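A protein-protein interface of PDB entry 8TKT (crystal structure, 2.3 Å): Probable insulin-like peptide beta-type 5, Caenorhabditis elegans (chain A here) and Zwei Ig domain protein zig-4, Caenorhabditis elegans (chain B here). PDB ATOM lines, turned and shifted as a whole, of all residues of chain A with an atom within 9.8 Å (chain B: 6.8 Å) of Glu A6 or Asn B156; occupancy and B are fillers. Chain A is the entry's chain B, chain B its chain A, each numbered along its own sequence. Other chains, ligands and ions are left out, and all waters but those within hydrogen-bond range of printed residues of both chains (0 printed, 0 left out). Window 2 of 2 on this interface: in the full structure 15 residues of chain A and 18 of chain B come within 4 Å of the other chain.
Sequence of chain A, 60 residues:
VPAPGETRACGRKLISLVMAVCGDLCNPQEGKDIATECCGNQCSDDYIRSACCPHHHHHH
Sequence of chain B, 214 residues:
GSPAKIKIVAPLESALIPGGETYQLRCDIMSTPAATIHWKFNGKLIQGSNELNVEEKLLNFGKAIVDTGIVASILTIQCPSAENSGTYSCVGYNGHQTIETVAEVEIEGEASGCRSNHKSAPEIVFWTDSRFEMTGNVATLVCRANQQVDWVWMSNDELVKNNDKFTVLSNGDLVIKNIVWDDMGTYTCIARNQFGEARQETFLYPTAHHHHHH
Arg A8 touches none of the printed residues of chain B.
Of the printed residues of chain B, Ala A9 touches Thr B186.
Of the printed residues of chain B, Cys A10 touches Phe B203.
Of the printed residues of chain B, Lys A13 touches Phe B203.
No residue of chain A comes within 4 Å of Ser B155.
Asn B156 touches just one residue of chain A: Glu A6.
No residue of chain A comes within 4 Å of Asp B157.
No residue of chain A comes within 4 Å of Glu B158.
Met B184 touches none of the printed residues of chain A.
Of chain A, only Glu A6 comes within 4 Å of Gly B185.
Of the printed residues of chain A, Phe B203 touches Cys A10 and Lys A13.
The nearest residue of chain B that does not touch Glu A6 is Met B184 (4.6 Å).
The nearest printed residue of chain B that does not touch Cys A10 is Met B184 (4.1 Å).
Among the printed residues, pairs that only touch across the chains: Glu A6 with Gly B185 (3.3 Å), Ala A9 with Thr B186 (3.8 Å), Cys A10 with Phe B203 (3.7 Å) and Lys A13 with Phe B203 (3.7 Å).
OD1 of Asn B156 sits close to OE2 of Glu A6, at 2.8 Å.
The backbone NH (N) of Thr B186 is in hydrogen-bond range of the side-chain carboxylate (OE1) of Glu A6 (3.0 Å).
SG of Cys A10 forms a disulfide with SG of Cys A39, at 2.0 Å.
Of the 16 printed residues of chain A, 4 touch a printed residue of chain B.
Printed residues of chain A that touch a printed residue of chain B: Glu A6, Ala A9, Cys A10 and Lys A13.
Of the 13 printed residues of chain B, 4 touch a printed residue of chain A.
Hydrophobic or aromatic side chains of chain B within 4 Å of the printed part of chain A: Phe B203.
Among the printed residues, 6 pairs touch across the chains.
Among the printed residues, no Asp or Glu carboxylate lies within 4 Å of a Lys or Arg side-chain nitrogen of the other chain.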
ATOM      1  N   ALA A   3      26.060  -4.725  -7.724  1.00  0.00           N
ATOM      2  CA  ALA A   3      25.879  -3.545  -6.887  1.00  0.00           C
ATOM      3  C   ALA A   3      26.567  -3.722  -5.538  1.00  0.00           C
ATOM      4  O   ALA A   3      26.567  -4.818  -4.975  1.00  0.00           O
ATOM      5  CB  ALA A   3      24.392  -3.253  -6.692  1.00  0.00           C
ATOM      6  N   PRO A   4      27.164  -2.649  -5.021  1.00  0.00           N
ATOM      7  CA  PRO A   4      27.687  -2.699  -3.653  1.00  0.00           C
ATOM      8  C   PRO A   4      26.540  -2.799  -2.660  1.00  0.00           C
ATOM      9  O   PRO A   4      25.477  -2.204  -2.853  1.00  0.00           O
ATOM     10  CB  PRO A   4      28.448  -1.376  -3.510  1.00  0.00           C
ATOM     11  CG  PRO A   4      27.805  -0.467  -4.499  1.00  0.00           C
ATOM     12  CD  PRO A   4      27.377  -1.335  -5.650  1.00  0.00           C
ATOM     13  N   GLY A   5      26.759  -3.583  -1.602  1.00  0.00           N
ATOM     14  CA  GLY A   5      25.711  -3.782  -0.613  1.00  0.00           C
ATOM     15  C   GLY A   5      25.208  -2.480  -0.021  1.00  0.00           C
ATOM     16  O   GLY A   5      24.019  -2.339   0.276  1.00  0.00           O
ATOM     17  N   GLU A   6      26.112  -1.515   0.168  1.00  0.00           N
ATOM     18  CA  GLU A   6      25.723  -0.215   0.705  1.00  0.00           C
ATOM     19  C   GLU A   6      24.713   0.489  -0.195  1.00  0.00           C
ATOM     20  O   GLU A   6      23.726   1.055   0.291  1.00  0.00           O
ATOM     21  CB  GLU A   6      26.961   0.660   0.890  1.00  0.00           C
ATOM     22  CG  GLU A   6      27.983   0.101   1.864  1.00  0.00           C
ATOM     23  CD  GLU A   6      27.587   0.319   3.310  1.00  0.00           C
ATOM     24  OE1 GLU A   6      26.719   1.181   3.565  1.00  0.00           O
ATOM     25  OE2 GLU A   6      28.143  -0.368   4.192  1.00  0.00           O
ATOM     26  N   THR A   7      24.928   0.446  -1.512  1.00  0.00           N
ATOM     27  CA  THR A   7      24.009   1.091  -2.442  1.00  0.00           C
ATOM     28  C   THR A   7      22.713   0.307  -2.600  1.00  0.00           C
ATOM     29  O   THR A   7      21.738   0.839  -3.143  1.00  0.00           O
ATOM     30  CB  THR A   7      24.702   1.286  -3.795  1.00  0.00           C
ATOM     31  OG1 THR A   7      25.959   1.942  -3.587  1.00  0.00           O
ATOM     32  CG2 THR A   7      23.866   2.157  -4.726  1.00  0.00           C
ATOM     33  N   ARG A   8      22.658  -0.914  -2.083  1.00  0.00           N
ATOM     34  CA  ARG A   8      21.482  -1.753  -2.239  1.00  0.00           C
ATOM     35  C   ARG A   8      20.618  -1.782  -0.989  1.00  0.00           C
ATOM     36  O   ARG A   8      19.393  -1.912  -1.102  1.00  0.00           O
ATOM     37  CB  ARG A   8      21.915  -3.172  -2.607  1.00  0.00           C
ATOM     38  CG  ARG A   8      20.813  -4.107  -3.042  1.00  0.00           C
ATOM     39  CD  ARG A   8      21.425  -5.334  -3.709  1.00  0.00           C
ATOM     40  NE  ARG A   8      22.169  -6.157  -2.760  1.00  0.00           N
ATOM     41  CZ  ARG A   8      23.486  -6.128  -2.604  1.00  0.00           C
ATOM     42  NH1 ARG A   8      24.273  -5.512  -3.471  1.00  0.00           N
ATOM     43  NH2 ARG A   8      24.032  -6.789  -1.587  1.00  0.00           N
ATOM     44  N   ALA A   9      21.217  -1.645   0.195  1.00  0.00           N
ATOM     45  CA  ALA A   9      20.407  -1.499   1.395  1.00  0.00           C
ATOM     46  C   ALA A   9      19.795  -0.109   1.463  1.00  0.00           C
ATOM     47  O   ALA A   9      18.678   0.051   1.967  1.00  0.00           O
ATOM     48  CB  ALA A   9      21.248  -1.778   2.640  1.00  0.00           C
ATOM     49  N   CYS A  10      20.522   0.895   0.963  1.00  0.00           N
ATOM     50  CA  CYS A  10      20.024   2.265   0.913  1.00  0.00           C
ATOM     51  C   CYS A  10      18.663   2.327   0.231  1.00  0.00           C
ATOM     52  O   CYS A  10      17.688   2.837   0.795  1.00  0.00           O
ATOM     53  CB  CYS A  10      21.041   3.152   0.194  1.00  0.00           C
ATOM     54  SG  CYS A  10      20.550   4.884   0.053  1.00  0.00           S
ATOM     55  N   GLY A  11      18.595   1.830  -1.006  1.00  0.00           N
ATOM     56  CA  GLY A  11      17.343   1.851  -1.746  1.00  0.00           C
ATOM     57  C   GLY A  11      16.220   1.139  -1.019  1.00  0.00           C
ATOM     58  O   GLY A  11      15.067   1.574  -1.055  1.00  0.00           O
ATOM     59  N   ARG A  12      16.542   0.027  -0.355  1.00  0.00           N
ATOM     60  CA  ARG A  12      15.527  -0.721   0.378  1.00  0.00           C
ATOM     61  C   ARG A  12      14.958   0.101   1.529  1.00  0.00           C
ATOM     62  O   ARG A  12      13.741   0.113   1.751  1.00  0.00           O
ATOM     63  CB  ARG A  12      16.130  -2.029   0.888  1.00  0.00           C
ATOM     64  CG  ARG A  12      15.247  -2.815   1.842  1.00  0.00           C
ATOM     65  CD  ARG A  12      15.771  -4.236   2.065  1.00  0.00           C
ATOM     66  NE  ARG A  12      17.208  -4.287   2.319  1.00  0.00           N
ATOM     67  CZ  ARG A  12      18.124  -4.636   1.425  1.00  0.00           C
ATOM     68  NH1 ARG A  12      17.794  -4.955   0.185  1.00  0.00           N
ATOM     69  NH2 ARG A  12      19.405  -4.661   1.784  1.00  0.00           N
ATOM     70  N   LYS A  13      15.821   0.791   2.279  1.00  0.00           N
ATOM     71  CA  LYS A  13      15.343   1.566   3.420  1.00  0.00           C
ATOM     72  C   LYS A  13      14.604   2.818   2.963  1.00  0.00           C
ATOM     73  O   LYS A  13      13.606   3.217   3.574  1.00  0.00           O
ATOM     74  CB  LYS A  13      16.510   1.933   4.333  1.00  0.00           C
ATOM     75  CG  LYS A  13      17.352   0.737   4.744  1.00  0.00           C
ATOM     76  CD  LYS A  13      16.560  -0.268   5.554  1.00  0.00           C
ATOM     77  CE  LYS A  13      17.481  -1.303   6.180  1.00  0.00           C
ATOM     78  NZ  LYS A  13      16.738  -2.530   6.576  1.00  0.00           N
ATOM     79  N   LEU A  14      15.087   3.452   1.891  1.00  0.00           N
ATOM     80  CA  LEU A  14      14.425   4.638   1.358  1.00  0.00           C
ATOM     81  C   LEU A  14      13.033   4.305   0.837  1.00  0.00           C
ATOM     82  O   LEU A  14      12.064   5.018   1.121  1.00  0.00           O
ATOM     83  CB  LEU A  14      15.277   5.254   0.250  1.00  0.00           C
ATOM     84  CG  LEU A  14      16.151   6.447   0.628  1.00  0.00           C
ATOM     85  CD1 LEU A  14      16.873   6.959  -0.593  1.00  0.00           C
ATOM     86  CD2 LEU A  14      15.290   7.541   1.216  1.00  0.00           C
ATOM     87  N   ALA A  35      14.354   6.334  -4.948  1.00  0.00           N
ATOM     88  CA  ALA A  35      15.358   5.629  -4.158  1.00  0.00           C
ATOM     89  C   ALA A  35      16.693   5.575  -4.888  1.00  0.00           C
ATOM     90  O   ALA A  35      17.750   5.761  -4.278  1.00  0.00           O
ATOM     91  CB  ALA A  35      14.868   4.221  -3.821  1.00  0.00           C
ATOM     92  N   CYS A  38      18.256   9.236  -4.764  1.00  0.00           N
ATOM     93  CA  CYS A  38      18.695   9.705  -3.459  1.00  0.00           C
ATOM     94  C   CYS A  38      19.752   8.819  -2.813  1.00  0.00           C
ATOM     95  O   CYS A  38      20.307   9.206  -1.779  1.00  0.00           O
ATOM     96  CB  CYS A  38      17.488   9.849  -2.532  1.00  0.00           C
ATOM     97  SG  CYS A  38      16.352  11.120  -3.098  1.00  0.00           S
ATOM     98  N   CYS A  39      20.049   7.655  -3.385  1.00  0.00           N
ATOM     99  CA  CYS A  39      21.156   6.839  -2.911  1.00  0.00           C
ATOM    100  C   CYS A  39      22.430   7.057  -3.713  1.00  0.00           C
ATOM    101  O   CYS A  39      23.502   6.625  -3.277  1.00  0.00           O
ATOM    102  CB  CYS A  39      20.772   5.356  -2.940  1.00  0.00           C
ATOM    103  SG  CYS A  39      19.528   4.932  -1.702  1.00  0.00           S
ATOM    104  N   GLY A  40      22.336   7.716  -4.863  1.00  0.00           N
ATOM    105  CA  GLY A  40      23.505   8.131  -5.608  1.00  0.00           C
ATOM    106  C   GLY A  40      23.959   9.518  -5.207  1.00  0.00           C
ATOM    107  O   GLY A  40      25.160   9.786  -5.104  1.00  0.00           O
ATOM    108  N   MET B 154      30.006  -1.677  13.789  1.00  0.00           N
ATOM    109  CA  MET B 154      30.826  -1.748  12.587  1.00  0.00           C
ATOM    110  C   MET B 154      30.238  -0.893  11.475  1.00  0.00           C
ATOM    111  O   MET B 154      29.027  -0.918  11.228  1.00  0.00           O
ATOM    112  CB  MET B 154      30.972  -3.191  12.097  1.00  0.00           C
ATOM    113  CG  MET B 154      32.107  -3.951  12.759  1.00  0.00           C
ATOM    114  SD  MET B 154      32.618  -5.387  11.797  1.00  0.00           S
ATOM    115  CE  MET B 154      31.087  -6.311  11.717  1.00  0.00           C
ATOM    116  N   SER B 155      31.108  -0.135  10.809  1.00  0.00           N
ATOM    117  CA  SER B 155      30.766   0.657   9.632  1.00  0.00           C
ATOM    118  C   SER B 155      31.613   0.195   8.452  1.00  0.00           C
ATOM    119  O   SER B 155      32.844   0.281   8.504  1.00  0.00           O
ATOM    120  CB  SER B 155      30.976   2.150   9.891  1.00  0.00           C
ATOM    121  OG  SER B 155      30.846   2.894   8.692  1.00  0.00           O
ATOM    122  N   ASN B 156      30.954  -0.285   7.394  1.00  0.00           N
ATOM    123  CA  ASN B 156      31.624  -0.687   6.152  1.00  0.00           C
ATOM    124  C   ASN B 156      32.747  -1.689   6.409  1.00  0.00           C
ATOM    125  O   ASN B 156      33.833  -1.599   5.829  1.00  0.00           O
ATOM    126  CB  ASN B 156      32.163   0.535   5.402  1.00  0.00           C
ATOM    127  CG  ASN B 156      31.124   1.627   5.237  1.00  0.00           C
ATOM    128  OD1 ASN B 156      29.925   1.390   5.384  1.00  0.00           O
ATOM    129  ND2 ASN B 156      31.583   2.837   4.931  1.00  0.00           N
ATOM    130  N   ASP B 157      32.489  -2.635   7.313  1.00  0.00           N
ATOM    131  CA  ASP B 157      33.398  -3.711   7.706  1.00  0.00           C
ATOM    132  C   ASP B 157      34.568  -3.213   8.544  1.00  0.00           C
ATOM    133  O   ASP B 157      35.494  -3.985   8.822  1.00  0.00           O
ATOM    134  CB  ASP B 157      33.927  -4.495   6.497  1.00  0.00           C
ATOM    135  N   GLU B 158      34.557  -1.948   8.958  1.00  0.00           N
ATOM    136  CA  GLU B 158      35.530  -1.419   9.900  1.00  0.00           C
ATOM    137  C   GLU B 158      34.876  -1.163  11.250  1.00  0.00           C
ATOM    138  O   GLU B 158      33.710  -0.761  11.324  1.00  0.00           O
ATOM    139  CB  GLU B 158      36.164  -0.124   9.382  1.00  0.00           C
ATOM    140  CG  GLU B 158      37.187  -0.331   8.280  1.00  0.00           C
ATOM    141  CD  GLU B 158      36.584  -0.204   6.895  1.00  0.00           C
ATOM    142  OE1 GLU B 158      35.754   0.707   6.687  1.00  0.00           O
ATOM    143  OE2 GLU B 158      36.937  -1.018   6.015  1.00  0.00           O
ATOM    144  N   LEU B 159      35.638  -1.404  12.311  1.00  0.00           N
ATOM    145  CA  LEU B 159      35.153  -1.178  13.663  1.00  0.00           C
ATOM    146  C   LEU B 159      34.977   0.314  13.922  1.00  0.00           C
ATOM    147  O   LEU B 159      35.787   1.135  13.483  1.00  0.00           O
ATOM    148  CB  LEU B 159      36.126  -1.779  14.677  1.00  0.00           C
ATOM    149  CG  LEU B 159      35.772  -1.587  16.151  1.00  0.00           C
ATOM    150  CD1 LEU B 159      34.663  -2.543  16.522  1.00  0.00           C
ATOM    151  CD2 LEU B 159      36.983  -1.788  17.047  1.00  0.00           C
ATOM    152  N   ASP B 182      28.997  11.423   3.820  1.00  0.00           N
ATOM    153  CA  ASP B 182      29.817  10.218   3.817  1.00  0.00           C
ATOM    154  C   ASP B 182      29.494   9.286   4.978  1.00  0.00           C
ATOM    155  O   ASP B 182      29.929   8.130   4.959  1.00  0.00           O
ATOM    156  CB  ASP B 182      31.301  10.584   3.841  1.00  0.00           C
ATOM    157  CG  ASP B 182      32.194   9.418   3.444  1.00  0.00           C
ATOM    158  OD1 ASP B 182      31.942   8.808   2.381  1.00  0.00           O
ATOM    159  OD2 ASP B 182      33.144   9.109   4.194  1.00  0.00           O
ATOM    160  N   MET B 184      26.518   8.280   5.446  1.00  0.00           N
ATOM    161  CA  MET B 184      25.386   7.503   4.966  1.00  0.00           C
ATOM    162  C   MET B 184      25.790   6.047   4.786  1.00  0.00           C
ATOM    163  O   MET B 184      26.873   5.746   4.280  1.00  0.00           O
ATOM    164  CB  MET B 184      24.887   8.078   3.639  1.00  0.00           C
ATOM    165  CG  MET B 184      23.585   7.487   3.123  1.00  0.00           C
ATOM    166  SD  MET B 184      23.863   5.987   2.159  1.00  0.00           S
ATOM    167  CE  MET B 184      24.739   6.659   0.749  1.00  0.00           C
ATOM    168  N   GLY B 185      24.916   5.144   5.203  1.00  0.00           N
ATOM    169  CA  GLY B 185      25.111   3.738   4.946  1.00  0.00           C
ATOM    170  C   GLY B 185      24.707   2.895   6.135  1.00  0.00           C
ATOM    171  O   GLY B 185      24.056   3.360   7.069  1.00  0.00           O
ATOM    172  N   THR B 186      25.128   1.635   6.090  1.00  0.00           N
ATOM    173  CA  THR B 186      24.734   0.635   7.071  1.00  0.00           C
ATOM    174  C   THR B 186      25.699   0.619   8.248  1.00  0.00           C
ATOM    175  O   THR B 186      26.921   0.619   8.063  1.00  0.00           O
ATOM    176  CB  THR B 186      24.678  -0.749   6.424  1.00  0.00           C
ATOM    177  OG1 THR B 186      23.818  -0.705   5.279  1.00  0.00           O
ATOM    178  CG2 THR B 186      24.149  -1.774   7.408  1.00  0.00           C
ATOM    179  N   TYR B 187      25.144   0.614   9.456  1.00  0.00           N
ATOM    180  CA  TYR B 187      25.910   0.440  10.682  1.00  0.00           C
ATOM    181  C   TYR B 187      25.390  -0.806  11.380  1.00  0.00           C
ATOM    182  O   TYR B 187      24.198  -0.895  11.689  1.00  0.00           O
ATOM    183  CB  TYR B 187      25.799   1.665  11.591  1.00  0.00           C
ATOM    184  CG  TYR B 187      26.430   2.900  10.995  1.00  0.00           C
ATOM    185  CD1 TYR B 187      25.796   3.604   9.979  1.00  0.00           C
ATOM    186  CD2 TYR B 187      27.671   3.349  11.427  1.00  0.00           C
ATOM    187  CE1 TYR B 187      26.368   4.730   9.424  1.00  0.00           C
ATOM    188  CE2 TYR B 187      28.254   4.473  10.874  1.00  0.00           C
ATOM    189  CZ  TYR B 187      27.597   5.158   9.872  1.00  0.00           C
ATOM    190  OH  TYR B 187      28.168   6.279   9.316  1.00  0.00           O
ATOM    191  N   THR B 188      26.276  -1.764  11.617  1.00  0.00           N
ATOM    192  CA  THR B 188      25.904  -3.015  12.256  1.00  0.00           C
ATOM    193  C   THR B 188      26.197  -2.914  13.744  1.00  0.00           C
ATOM    194  O   THR B 188      27.289  -2.495  14.139  1.00  0.00           O
ATOM    195  CB  THR B 188      26.674  -4.187  11.645  1.00  0.00           C
ATOM    196  OG1 THR B 188      26.577  -4.125  10.218  1.00  0.00           O
ATOM    197  CG2 THR B 188      26.104  -5.516  12.129  1.00  0.00           C
ATOM    198  N   PHE B 203      20.555   1.777   9.618  1.00  0.00           N
ATOM    199  CA  PHE B 203      20.845   2.589   8.446  1.00  0.00           C
ATOM    200  C   PHE B 203      20.687   4.063   8.779  1.00  0.00           C
ATOM    201  O   PHE B 203      19.743   4.457   9.468  1.00  0.00           O
ATOM    202  CB  PHE B 203      19.934   2.213   7.271  1.00  0.00           C
ATOM    203  CG  PHE B 203      20.141   3.061   6.050  1.00  0.00           C
ATOM    204  CD1 PHE B 203      21.235   2.852   5.226  1.00  0.00           C
ATOM    205  CD2 PHE B 203      19.239   4.061   5.720  1.00  0.00           C
ATOM    206  CE1 PHE B 203      21.434   3.630   4.101  1.00  0.00           C
ATOM    207  CE2 PHE B 203      19.429   4.842   4.594  1.00  0.00           C
ATOM    208  CZ  PHE B 203      20.529   4.627   3.784  1.00  0.00           C
